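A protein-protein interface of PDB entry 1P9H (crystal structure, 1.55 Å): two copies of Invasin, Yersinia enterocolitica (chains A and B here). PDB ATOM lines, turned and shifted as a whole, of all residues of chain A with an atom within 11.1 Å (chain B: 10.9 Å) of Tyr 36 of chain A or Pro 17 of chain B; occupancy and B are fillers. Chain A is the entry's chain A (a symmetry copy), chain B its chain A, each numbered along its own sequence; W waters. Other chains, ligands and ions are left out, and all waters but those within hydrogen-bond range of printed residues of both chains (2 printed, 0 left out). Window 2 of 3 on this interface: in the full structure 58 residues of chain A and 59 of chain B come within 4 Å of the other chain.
Among the printed residues, pairs that only touch across the chains: Pro 26 of chain A with Ala 21 of chain B, Asn 27 of chain A with Val 22 of chain B, Pro 26 of chain A with Leu 19 of chain B, Ala 28 of chain A with Leu 19 of chain B, Pro 30 of chain A with Ala 52 of chain B, Pro 30 of chain A with Thr 20 of chain B, Leu 48 of chain A with Leu 19 of chain B, Pro 26 of chain A with Thr 20 of chain B, Asp 29 of chain A with Pro 17 of chain B, Tyr 36 of chain A with Pro 17 of chain B, Glu 35 of chain A with Ile 24 of chain B, Leu 48 of chain A with Thr 20 of chain B, Asp 29 of chain A with Leu 19 of chain B, Ile 24 of chain A with Ile 24 of chain B, Pro 26 of chain A with Val 22 of chain B, Ile 24 of chain A with Val 22 of chain B, Ser 25 of chain A with Val 22 of chain B, Asn 27 of chain A with Leu 19 of chain B, Tyr 36 of chain A with Leu 19 of chain B and Ala 28 of chain A with Gln 23 of chain B.
Of the 15 printed residues of chain B, 10 touch a printed residue of chain A.
Printed residues of chain B that touch a printed residue of chain A: Pro 17, Asn 18, Leu 19, Thr 20, Ala 21, Val 22, Gln 23, Ile 24, Ser 25 and Ala 52.
Hydrophobic or aromatic side chains of chain A that line the printed part of chain B: Ile 24, Pro 26, Ala 28, Pro 30, Tyr 36 and Leu 48.
Among the printed residues, 28 pairs touch across the chains.
Among the printed residues, no Asp or Glu carboxylate lies within 4 Å of a Lys or Arg side-chain nitrogen of the other chain.
O of Val 22 of chain B lies within hydrogen-bond range of N of Ala 59 of chain B (2.9 Å).
The side-chain amide nitrogen (NE2) of Gln 23 of chain B lies close to the backbone carbonyl oxygen (O) of Ala 50 of chain B (3.2 Å).
The backbone NH of Ile 24 of chain B is in hydrogen-bond range of the backbone carbonyl oxygen of Ala 59 of chain B, at 2.8 Å.
N of Ala 50 of chain B lies within hydrogen-bond range of OG of Ser 25 of chain B (2.8 Å).
O of Asn 27 of chain A sits at hydrogen-bond distance from N of Tyr 36 of chain A, at 2.7 Å.
OD1 of Asp 29 of chain A lies within hydrogen-bond range of N of Ala 31 of chain A, 2.8 Å away.
N of Asn 18 of chain B sits at hydrogen-bond distance from OD2 of Asp 29 of chain A, 2.7 Å away.
The backbone carbonyl oxygen of Ala 28 of chain A is in hydrogen-bond range of the backbone NH of Thr 20 of chain B.
The backbone carbonyl oxygen (O) of Ala 21 of chain B is in hydrogen-bond range of the backbone NH (N) of Asn 27 of chain A (2.9 Å).
The backbone NH of Ala 28 of chain A lies within hydrogen-bond range of the backbone carbonyl oxygen of Ala 21 of chain B, 3.1 Å away.
The backbone NH (N) of Gln 23 of chain B sits at hydrogen-bond distance from the side-chain amide oxygen (OD1) of Asn 27 of chain A (2.8 Å).
NE2 of Gln 23 of chain B sits at hydrogen-bond distance from O of Gly 33 of chain A.
The side-chain amide nitrogen (NE2) of Gln 23 of chain B sits at hydrogen-bond distance from the side-chain carboxylate (OE1) of Glu 35 of chain A, at 3.0 Å.
The side-chain hydroxyl (OG) of Ser 25 of chain B lies within hydrogen-bond range of the side-chain carboxylate (OE1) of Glu 35 of chain A, at 2.8 Å.
Ile 24 of chain B touches its own counterpart, Ile 24 of chain A.
4 positions are printed for both chains.
Of the 28 pairs that touch across the chains among the printed residues, 1 has its exchanged pair printed and touching as well.
Of the printed residues of chain B, Pro 26 of chain A touches Leu 19, Thr 20, Ala 21 and Val 22.
Of the printed residues of chain B, Ala 28 of chain A touches Leu 19 (3.4 Å), Thr 20 (3.2 Å), Ala 21 (3.1 Å) and Gln 23 (3.998 Å).
No residue of chain B comes within 4 Å of Leu 34 of chain A.
Glu 35 of chain A touches just these residues of chain B: Gln 23 (3.0 Å), Ile 24 (3.7 Å) and Ser 25 (2.8 Å).
Of the printed residues of chain B, Tyr 36 of chain A touches Pro 17 and Leu 19.
Pro 17 of chain B touches just these residues of chain A: Asp 29 (3.6 Å) and Tyr 36 (3.7 Å).
Asn 27 of chain B touches none of the printed residues of chain A.
The nearest residue of chain A that does not touch Pro 17 of chain B is Leu 32 of chain A (4.04 Å).
The nearest printed residue of chain A that does not touch Thr 20 of chain B is Asp 29 of chain A (4.9 Å).
Water W2 lies within hydrogen-bond range of the backbone carbonyl oxygen of Ser 25 of chain B (2.8 Å) and the side-chain carboxylate of Glu 35 of chain A (3.5 Å).
Water W1 lies within hydrogen-bond range of the side-chain amide oxygen (OD1) of Asn 49 of chain B (3.0 Å) and the side-chain carboxylate (OE1) of Glu 35 of chain A (3.0 Å).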
ATOM      1  N   ILE A  24      -0.892  35.374  21.870  1.00  0.00           N
ATOM      2  CA  ILE A  24       0.137  34.359  21.733  1.00  0.00           C
ATOM      3  C   ILE A  24       0.825  34.425  20.380  1.00  0.00           C
ATOM      4  O   ILE A  24       0.278  33.989  19.364  1.00  0.00           O
ATOM      5  CB  ILE A  24      -0.451  32.945  21.931  1.00  0.00           C
ATOM      6  CG1 ILE A  24      -1.139  32.860  23.299  1.00  0.00           C
ATOM      7  CG2 ILE A  24       0.655  31.901  21.828  1.00  0.00           C
ATOM      8  CD1 ILE A  24      -1.871  31.559  23.547  1.00  0.00           C
ATOM      9  N   SER A  25       2.025  34.995  20.374  1.00  0.00           N
ATOM     10  CA  SER A  25       2.821  35.111  19.161  1.00  0.00           C
ATOM     11  C   SER A  25       3.576  33.797  18.961  1.00  0.00           C
ATOM     12  O   SER A  25       3.640  32.971  19.875  1.00  0.00           O
ATOM     13  CB  SER A  25       3.814  36.271  19.296  1.00  0.00           C
ATOM     14  OG  SER A  25       3.135  37.509  19.426  1.00  0.00           O
ATOM     15  N   PRO A  26       4.150  33.579  17.766  1.00  0.00           N
ATOM     16  CA  PRO A  26       4.892  32.344  17.498  1.00  0.00           C
ATOM     17  C   PRO A  26       5.874  32.018  18.618  1.00  0.00           C
ATOM     18  O   PRO A  26       6.616  32.888  19.077  1.00  0.00           O
ATOM     19  CB  PRO A  26       5.587  32.651  16.177  1.00  0.00           C
ATOM     20  CG  PRO A  26       4.553  33.470  15.469  1.00  0.00           C
ATOM     21  CD  PRO A  26       4.082  34.421  16.556  1.00  0.00           C
ATOM     22  N   ASN A  27       5.872  30.762  19.052  1.00  0.00           N
ATOM     23  CA  ASN A  27       6.751  30.327  20.133  1.00  0.00           C
ATOM     24  C   ASN A  27       7.549  29.088  19.751  1.00  0.00           C
ATOM     25  O   ASN A  27       8.178  28.464  20.607  1.00  0.00           O
ATOM     26  CB  ASN A  27       5.923  30.023  21.384  1.00  0.00           C
ATOM     27  CG  ASN A  27       5.134  28.732  21.258  1.00  0.00           C
ATOM     28  OD1 ASN A  27       4.726  28.348  20.164  1.00  0.00           O
ATOM     29  ND2 ASN A  27       4.910  28.056  22.382  1.00  0.00           N
ATOM     30  N   ALA A  28       7.535  28.731  18.471  1.00  0.00           N
ATOM     31  CA  ALA A  28       8.255  27.545  18.032  1.00  0.00           C
ATOM     32  C   ALA A  28       8.742  27.603  16.593  1.00  0.00           C
ATOM     33  O   ALA A  28       8.150  28.270  15.745  1.00  0.00           O
ATOM     34  CB  ALA A  28       7.373  26.314  18.222  1.00  0.00           C
ATOM     35  N   ASP A  29       9.840  26.899  16.336  1.00  0.00           N
ATOM     36  CA  ASP A  29      10.408  26.807  15.000  1.00  0.00           C
ATOM     37  C   ASP A  29      10.007  25.409  14.545  1.00  0.00           C
ATOM     38  O   ASP A  29      10.499  24.412  15.076  1.00  0.00           O
ATOM     39  CB  ASP A  29      11.933  26.921  15.047  1.00  0.00           C
ATOM     40  CG  ASP A  29      12.559  26.932  13.664  1.00  0.00           C
ATOM     41  OD1 ASP A  29      12.212  26.052  12.846  1.00  0.00           O
ATOM     42  OD2 ASP A  29      13.400  27.817  13.395  1.00  0.00           O
ATOM     43  N   PRO A  30       9.098  25.315  13.565  1.00  0.00           N
ATOM     44  CA  PRO A  30       8.637  24.021  13.054  1.00  0.00           C
ATOM     45  C   PRO A  30       9.741  23.112  12.526  1.00  0.00           C
ATOM     46  O   PRO A  30       9.524  21.917  12.324  1.00  0.00           O
ATOM     47  CB  PRO A  30       7.630  24.418  11.974  1.00  0.00           C
ATOM     48  CG  PRO A  30       8.154  25.733  11.493  1.00  0.00           C
ATOM     49  CD  PRO A  30       8.521  26.421  12.782  1.00  0.00           C
ATOM     50  N   ALA A  31      10.923  23.677  12.312  1.00  0.00           N
ATOM     51  CA  ALA A  31      12.055  22.905  11.810  1.00  0.00           C
ATOM     52  C   ALA A  31      12.834  22.274  12.961  1.00  0.00           C
ATOM     53  O   ALA A  31      13.752  21.484  12.740  1.00  0.00           O
ATOM     54  CB  ALA A  31      12.973  23.799  10.987  1.00  0.00           C
ATOM     55  N   LEU A  32      12.462  22.623  14.189  1.00  0.00           N
ATOM     56  CA  LEU A  32      13.126  22.089  15.372  1.00  0.00           C
ATOM     57  C   LEU A  32      12.128  21.403  16.300  1.00  0.00           C
ATOM     58  O   LEU A  32      12.490  20.505  17.061  1.00  0.00           O
ATOM     59  CB  LEU A  32      13.847  23.211  16.124  1.00  0.00           C
ATOM     60  CG  LEU A  32      14.883  24.006  15.321  1.00  0.00           C
ATOM     61  CD1 LEU A  32      15.490  25.085  16.204  1.00  0.00           C
ATOM     62  CD2 LEU A  32      15.962  23.071  14.798  1.00  0.00           C
ATOM     63  N   GLY A  33      10.873  21.835  16.236  1.00  0.00           N
ATOM     64  CA  GLY A  33       9.837  21.242  17.064  1.00  0.00           C
ATOM     65  C   GLY A  33       9.914  21.597  18.537  1.00  0.00           C
ATOM     66  O   GLY A  33       9.288  20.940  19.371  1.00  0.00           O
ATOM     67  N   LEU A  34      10.677  22.636  18.865  1.00  0.00           N
ATOM     68  CA  LEU A  34      10.819  23.064  20.251  1.00  0.00           C
ATOM     69  C   LEU A  34      10.011  24.323  20.533  1.00  0.00           C
ATOM     70  O   LEU A  34      10.174  25.342  19.862  1.00  0.00           O
ATOM     71  CB  LEU A  34      12.292  23.318  20.582  1.00  0.00           C
ATOM     72  CG  LEU A  34      13.214  22.098  20.565  1.00  0.00           C
ATOM     73  CD1 LEU A  34      14.639  22.532  20.863  1.00  0.00           C
ATOM     74  CD2 LEU A  34      12.740  21.080  21.591  1.00  0.00           C
ATOM     75  N   GLU A  35       9.135  24.246  21.530  1.00  0.00           N
ATOM     76  CA  GLU A  35       8.305  25.385  21.903  1.00  0.00           C
ATOM     77  C   GLU A  35       8.929  26.114  23.089  1.00  0.00           C
ATOM     78  O   GLU A  35       9.409  25.488  24.035  1.00  0.00           O
ATOM     79  CB  GLU A  35       6.888  24.914  22.250  1.00  0.00           C
ATOM     80  CG  GLU A  35       6.778  24.117  23.538  1.00  0.00           C
ATOM     81  CD  GLU A  35       5.463  23.365  23.648  1.00  0.00           C
ATOM     82  OE1 GLU A  35       5.299  22.351  22.933  1.00  0.00           O
ATOM     83  OE2 GLU A  35       4.594  23.788  24.444  1.00  0.00           O
ATOM     84  N   TYR A  36       8.930  27.442  23.027  1.00  0.00           N
ATOM     85  CA  TYR A  36       9.498  28.253  24.095  1.00  0.00           C
ATOM     86  C   TYR A  36       8.401  28.932  24.907  1.00  0.00           C
ATOM     87  O   TYR A  36       8.583  29.119  26.109  1.00  0.00           O
ATOM     88  CB  TYR A  36      10.440  29.312  23.514  1.00  0.00           C
ATOM     89  CG  TYR A  36      11.593  28.745  22.713  1.00  0.00           C
ATOM     90  CD1 TYR A  36      11.400  28.247  21.423  1.00  0.00           C
ATOM     91  CD2 TYR A  36      12.881  28.701  23.247  1.00  0.00           C
ATOM     92  CE1 TYR A  36      12.462  27.722  20.686  1.00  0.00           C
ATOM     93  CE2 TYR A  36      13.947  28.177  22.522  1.00  0.00           C
ATOM     94  CZ  TYR A  36      13.732  27.691  21.244  1.00  0.00           C
ATOM     95  OH  TYR A  36      14.792  27.183  20.525  1.00  0.00           O
ATOM     96  N   GLY A  47       8.465  40.431  12.983  1.00  0.00           N
ATOM     97  CA  GLY A  47       7.217  41.133  12.757  1.00  0.00           C
ATOM     98  C   GLY A  47       6.035  40.190  12.642  1.00  0.00           C
ATOM     99  O   GLY A  47       5.044  40.504  11.983  1.00  0.00           O
ATOM    100  N   LEU A  48       6.136  39.032  13.287  1.00  0.00           N
ATOM    101  CA  LEU A  48       5.065  38.042  13.248  1.00  0.00           C
ATOM    102  C   LEU A  48       4.243  38.036  14.531  1.00  0.00           C
ATOM    103  O   LEU A  48       3.458  37.119  14.768  1.00  0.00           O
ATOM    104  CB  LEU A  48       5.644  36.644  13.022  1.00  0.00           C
ATOM    105  CG  LEU A  48       6.465  36.413  11.751  1.00  0.00           C
ATOM    106  CD1 LEU A  48       6.883  34.953  11.692  1.00  0.00           C
ATOM    107  CD2 LEU A  48       5.648  36.784  10.523  1.00  0.00           C
ATOM    108  N   PRO B  17      16.936  30.418  15.974  1.00  0.00           N
ATOM    109  CA  PRO B  17      15.667  29.750  15.604  1.00  0.00           C
ATOM    110  C   PRO B  17      14.649  30.767  15.096  1.00  0.00           C
ATOM    111  O   PRO B  17      14.485  31.836  15.682  1.00  0.00           O
ATOM    112  CB  PRO B  17      15.149  29.057  16.855  1.00  0.00           C
ATOM    113  CG  PRO B  17      16.438  28.864  17.654  1.00  0.00           C
ATOM    114  CD  PRO B  17      17.252  30.135  17.386  1.00  0.00           C
ATOM    115  N   ASN B  18      13.973  30.429  14.003  1.00  0.00           N
ATOM    116  CA  ASN B  18      12.967  31.312  13.427  1.00  0.00           C
ATOM    117  C   ASN B  18      11.587  30.860  13.893  1.00  0.00           C
ATOM    118  O   ASN B  18      11.063  29.844  13.431  1.00  0.00           O
ATOM    119  CB  ASN B  18      13.047  31.280  11.898  1.00  0.00           C
ATOM    120  CG  ASN B  18      12.123  32.289  11.244  1.00  0.00           C
ATOM    121  OD1 ASN B  18      12.153  33.477  11.569  1.00  0.00           O
ATOM    122  ND2 ASN B  18      11.300  31.821  10.313  1.00  0.00           N
ATOM    123  N   LEU B  19      11.006  31.618  14.816  1.00  0.00           N
ATOM    124  CA  LEU B  19       9.695  31.291  15.363  1.00  0.00           C
ATOM    125  C   LEU B  19       8.558  31.775  14.469  1.00  0.00           C
ATOM    126  O   LEU B  19       8.311  32.977  14.355  1.00  0.00           O
ATOM    127  CB  LEU B  19       9.550  31.901  16.761  1.00  0.00           C
ATOM    128  CG  LEU B  19      10.706  31.639  17.730  1.00  0.00           C
ATOM    129  CD1 LEU B  19      10.408  32.303  19.063  1.00  0.00           C
ATOM    130  CD2 LEU B  19      10.910  30.143  17.910  1.00  0.00           C
ATOM    131  N   THR B  20       7.867  30.831  13.836  1.00  0.00           N
ATOM    132  CA  THR B  20       6.752  31.157  12.956  1.00  0.00           C
ATOM    133  C   THR B  20       5.494  30.393  13.349  1.00  0.00           C
ATOM    134  O   THR B  20       4.393  30.738  12.921  1.00  0.00           O
ATOM    135  CB  THR B  20       7.066  30.802  11.490  1.00  0.00           C
ATOM    136  OG1 THR B  20       7.312  29.393  11.383  1.00  0.00           O
ATOM    137  CG2 THR B  20       8.288  31.571  11.000  1.00  0.00           C
ATOM    138  N   ALA B  21       5.657  29.362  14.169  1.00  0.00           N
ATOM    139  CA  ALA B  21       4.524  28.544  14.580  1.00  0.00           C
ATOM    140  C   ALA B  21       4.181  28.670  16.055  1.00  0.00           C
ATOM    141  O   ALA B  21       4.967  29.184  16.848  1.00  0.00           O
ATOM    142  CB  ALA B  21       4.802  27.081  14.243  1.00  0.00           C
ATOM    143  N   VAL B  22       2.985  28.212  16.409  1.00  0.00           N
ATOM    144  CA  VAL B  22       2.539  28.220  17.794  1.00  0.00           C
ATOM    145  C   VAL B  22       2.315  26.770  18.187  1.00  0.00           C
ATOM    146  O   VAL B  22       1.509  26.067  17.574  1.00  0.00           O
ATOM    147  CB  VAL B  22       1.212  28.989  17.985  1.00  0.00           C
ATOM    148  CG1 VAL B  22       0.691  28.775  19.410  1.00  0.00           C
ATOM    149  CG2 VAL B  22       1.427  30.476  17.719  1.00  0.00           C
ATOM    150  N   GLN B  23       3.047  26.321  19.198  1.00  0.00           N
ATOM    151  CA  GLN B  23       2.925  24.954  19.675  1.00  0.00           C
ATOM    152  C   GLN B  23       2.717  25.027  21.174  1.00  0.00           C
ATOM    153  O   GLN B  23       3.588  25.495  21.907  1.00  0.00           O
ATOM    154  CB  GLN B  23       4.193  24.166  19.344  1.00  0.00           C
ATOM    155  CG  GLN B  23       4.156  22.699  19.735  1.00  0.00           C
ATOM    156  CD  GLN B  23       5.402  21.962  19.279  1.00  0.00           C
ATOM    157  OE1 GLN B  23       5.610  21.751  18.083  1.00  0.00           O
ATOM    158  NE2 GLN B  23       6.247  21.581  20.231  1.00  0.00           N
ATOM    159  N   ILE B  24       1.552  24.582  21.629  1.00  0.00           N
ATOM    160  CA  ILE B  24       1.244  24.628  23.048  1.00  0.00           C
ATOM    161  C   ILE B  24       0.874  23.260  23.595  1.00  0.00           C
ATOM    162  O   ILE B  24      -0.237  22.767  23.384  1.00  0.00           O
ATOM    163  CB  ILE B  24       0.090  25.614  23.331  1.00  0.00           C
ATOM    164  CG1 ILE B  24       0.455  27.003  22.794  1.00  0.00           C
ATOM    165  CG2 ILE B  24      -0.183  25.680  24.829  1.00  0.00           C
ATOM    166  CD1 ILE B  24      -0.660  28.021  22.895  1.00  0.00           C
ATOM    167  N   SER B  25       1.826  22.642  24.285  1.00  0.00           N
ATOM    168  CA  SER B  25       1.617  21.337  24.895  1.00  0.00           C
ATOM    169  C   SER B  25       0.940  21.549  26.248  1.00  0.00           C
ATOM    170  O   SER B  25       0.888  22.674  26.749  1.00  0.00           O
ATOM    171  CB  SER B  25       2.963  20.628  25.086  1.00  0.00           C
ATOM    172  OG  SER B  25       3.584  20.371  23.838  1.00  0.00           O
ATOM    173  N   ASN B  27      -0.068  22.338  29.833  1.00  0.00           N
ATOM    174  CA  ASN B  27       0.622  23.186  30.800  1.00  0.00           C
ATOM    175  C   ASN B  27      -0.081  23.197  32.149  1.00  0.00           C
ATOM    176  O   ASN B  27       0.239  24.016  33.012  1.00  0.00           O
ATOM    177  CB  ASN B  27       0.706  24.618  30.265  1.00  0.00           C
ATOM    178  CG  ASN B  27      -0.632  25.335  30.317  1.00  0.00           C
ATOM    179  OD1 ASN B  27      -1.684  24.712  30.193  1.00  0.00           O
ATOM    180  ND2 ASN B  27      -0.598  26.653  30.493  1.00  0.00           N
ATOM    181  N   TYR B  36       1.188  26.294  34.186  1.00  0.00           N
ATOM    182  CA  TYR B  36       2.600  26.652  34.209  1.00  0.00           C
ATOM    183  C   TYR B  36       3.007  27.346  32.913  1.00  0.00           C
ATOM    184  O   TYR B  36       3.876  28.215  32.954  1.00  0.00           O
ATOM    185  CB  TYR B  36       3.461  25.404  34.417  1.00  0.00           C
ATOM    186  CG  TYR B  36       3.164  24.652  35.698  1.00  0.00           C
ATOM    187  CD1 TYR B  36       2.026  23.854  35.818  1.00  0.00           C
ATOM    188  CD2 TYR B  36       4.022  24.742  36.795  1.00  0.00           C
ATOM    189  CE1 TYR B  36       1.751  23.163  36.998  1.00  0.00           C
ATOM    190  CE2 TYR B  36       3.755  24.060  37.978  1.00  0.00           C
ATOM    191  CZ  TYR B  36       2.621  23.273  38.074  1.00  0.00           C
ATOM    192  OH  TYR B  36       2.368  22.589  39.243  1.00  0.00           O
ATOM    193  N   ASN B  49       3.054  15.871  24.092  1.00  0.00           N
ATOM    194  CA  ASN B  49       3.453  17.104  23.426  1.00  0.00           C
ATOM    195  C   ASN B  49       2.662  17.391  22.157  1.00  0.00           C
ATOM    196  O   ASN B  49       2.311  16.480  21.405  1.00  0.00           O
ATOM    197  CB  ASN B  49       4.944  17.070  23.075  1.00  0.00           C
ATOM    198  CG  ASN B  49       5.836  17.391  24.258  1.00  0.00           C
ATOM    199  OD1 ASN B  49       7.058  17.437  24.127  1.00  0.00           O
ATOM    200  ND2 ASN B  49       5.231  17.620  25.415  1.00  0.00           N
ATOM    201  N   ALA B  50       2.381  18.671  21.936  1.00  0.00           N
ATOM    202  CA  ALA B  50       1.678  19.112  20.741  1.00  0.00           C
ATOM    203  C   ALA B  50       2.765  19.236  19.685  1.00  0.00           C
ATOM    204  O   ALA B  50       3.947  19.346  20.020  1.00  0.00           O
ATOM    205  CB  ALA B  50       1.017  20.460  20.985  1.00  0.00           C
ATOM    206  N   ALA B  52       3.527  21.365  16.067  1.00  0.00           N
ATOM    207  CA  ALA B  52       3.231  22.309  14.995  1.00  0.00           C
ATOM    208  C   ALA B  52       4.384  22.162  14.005  1.00  0.00           C
ATOM    209  O   ALA B  52       5.424  22.806  14.150  1.00  0.00           O
ATOM    210  CB  ALA B  52       3.173  23.731  15.543  1.00  0.00           C
ATOM    211  N   ALA B  59      -0.658  24.365  16.840  1.00  0.00           N
ATOM    212  CA  ALA B  59      -1.063  23.093  17.433  1.00  0.00           C
ATOM    213  C   ALA B  59      -1.181  23.311  18.933  1.00  0.00           C
ATOM    214  O   ALA B  59      -0.197  23.644  19.596  1.00  0.00           O
ATOM    215  CB  ALA B  59      -0.033  22.008  17.133  1.00  0.00           C
HETATM  216  O   HOH W   1       7.457  20.329  23.447  1.00  0.00           O
HETATM  217  O   HOH W   2       2.734  24.750  27.219  1.00  0.00           O
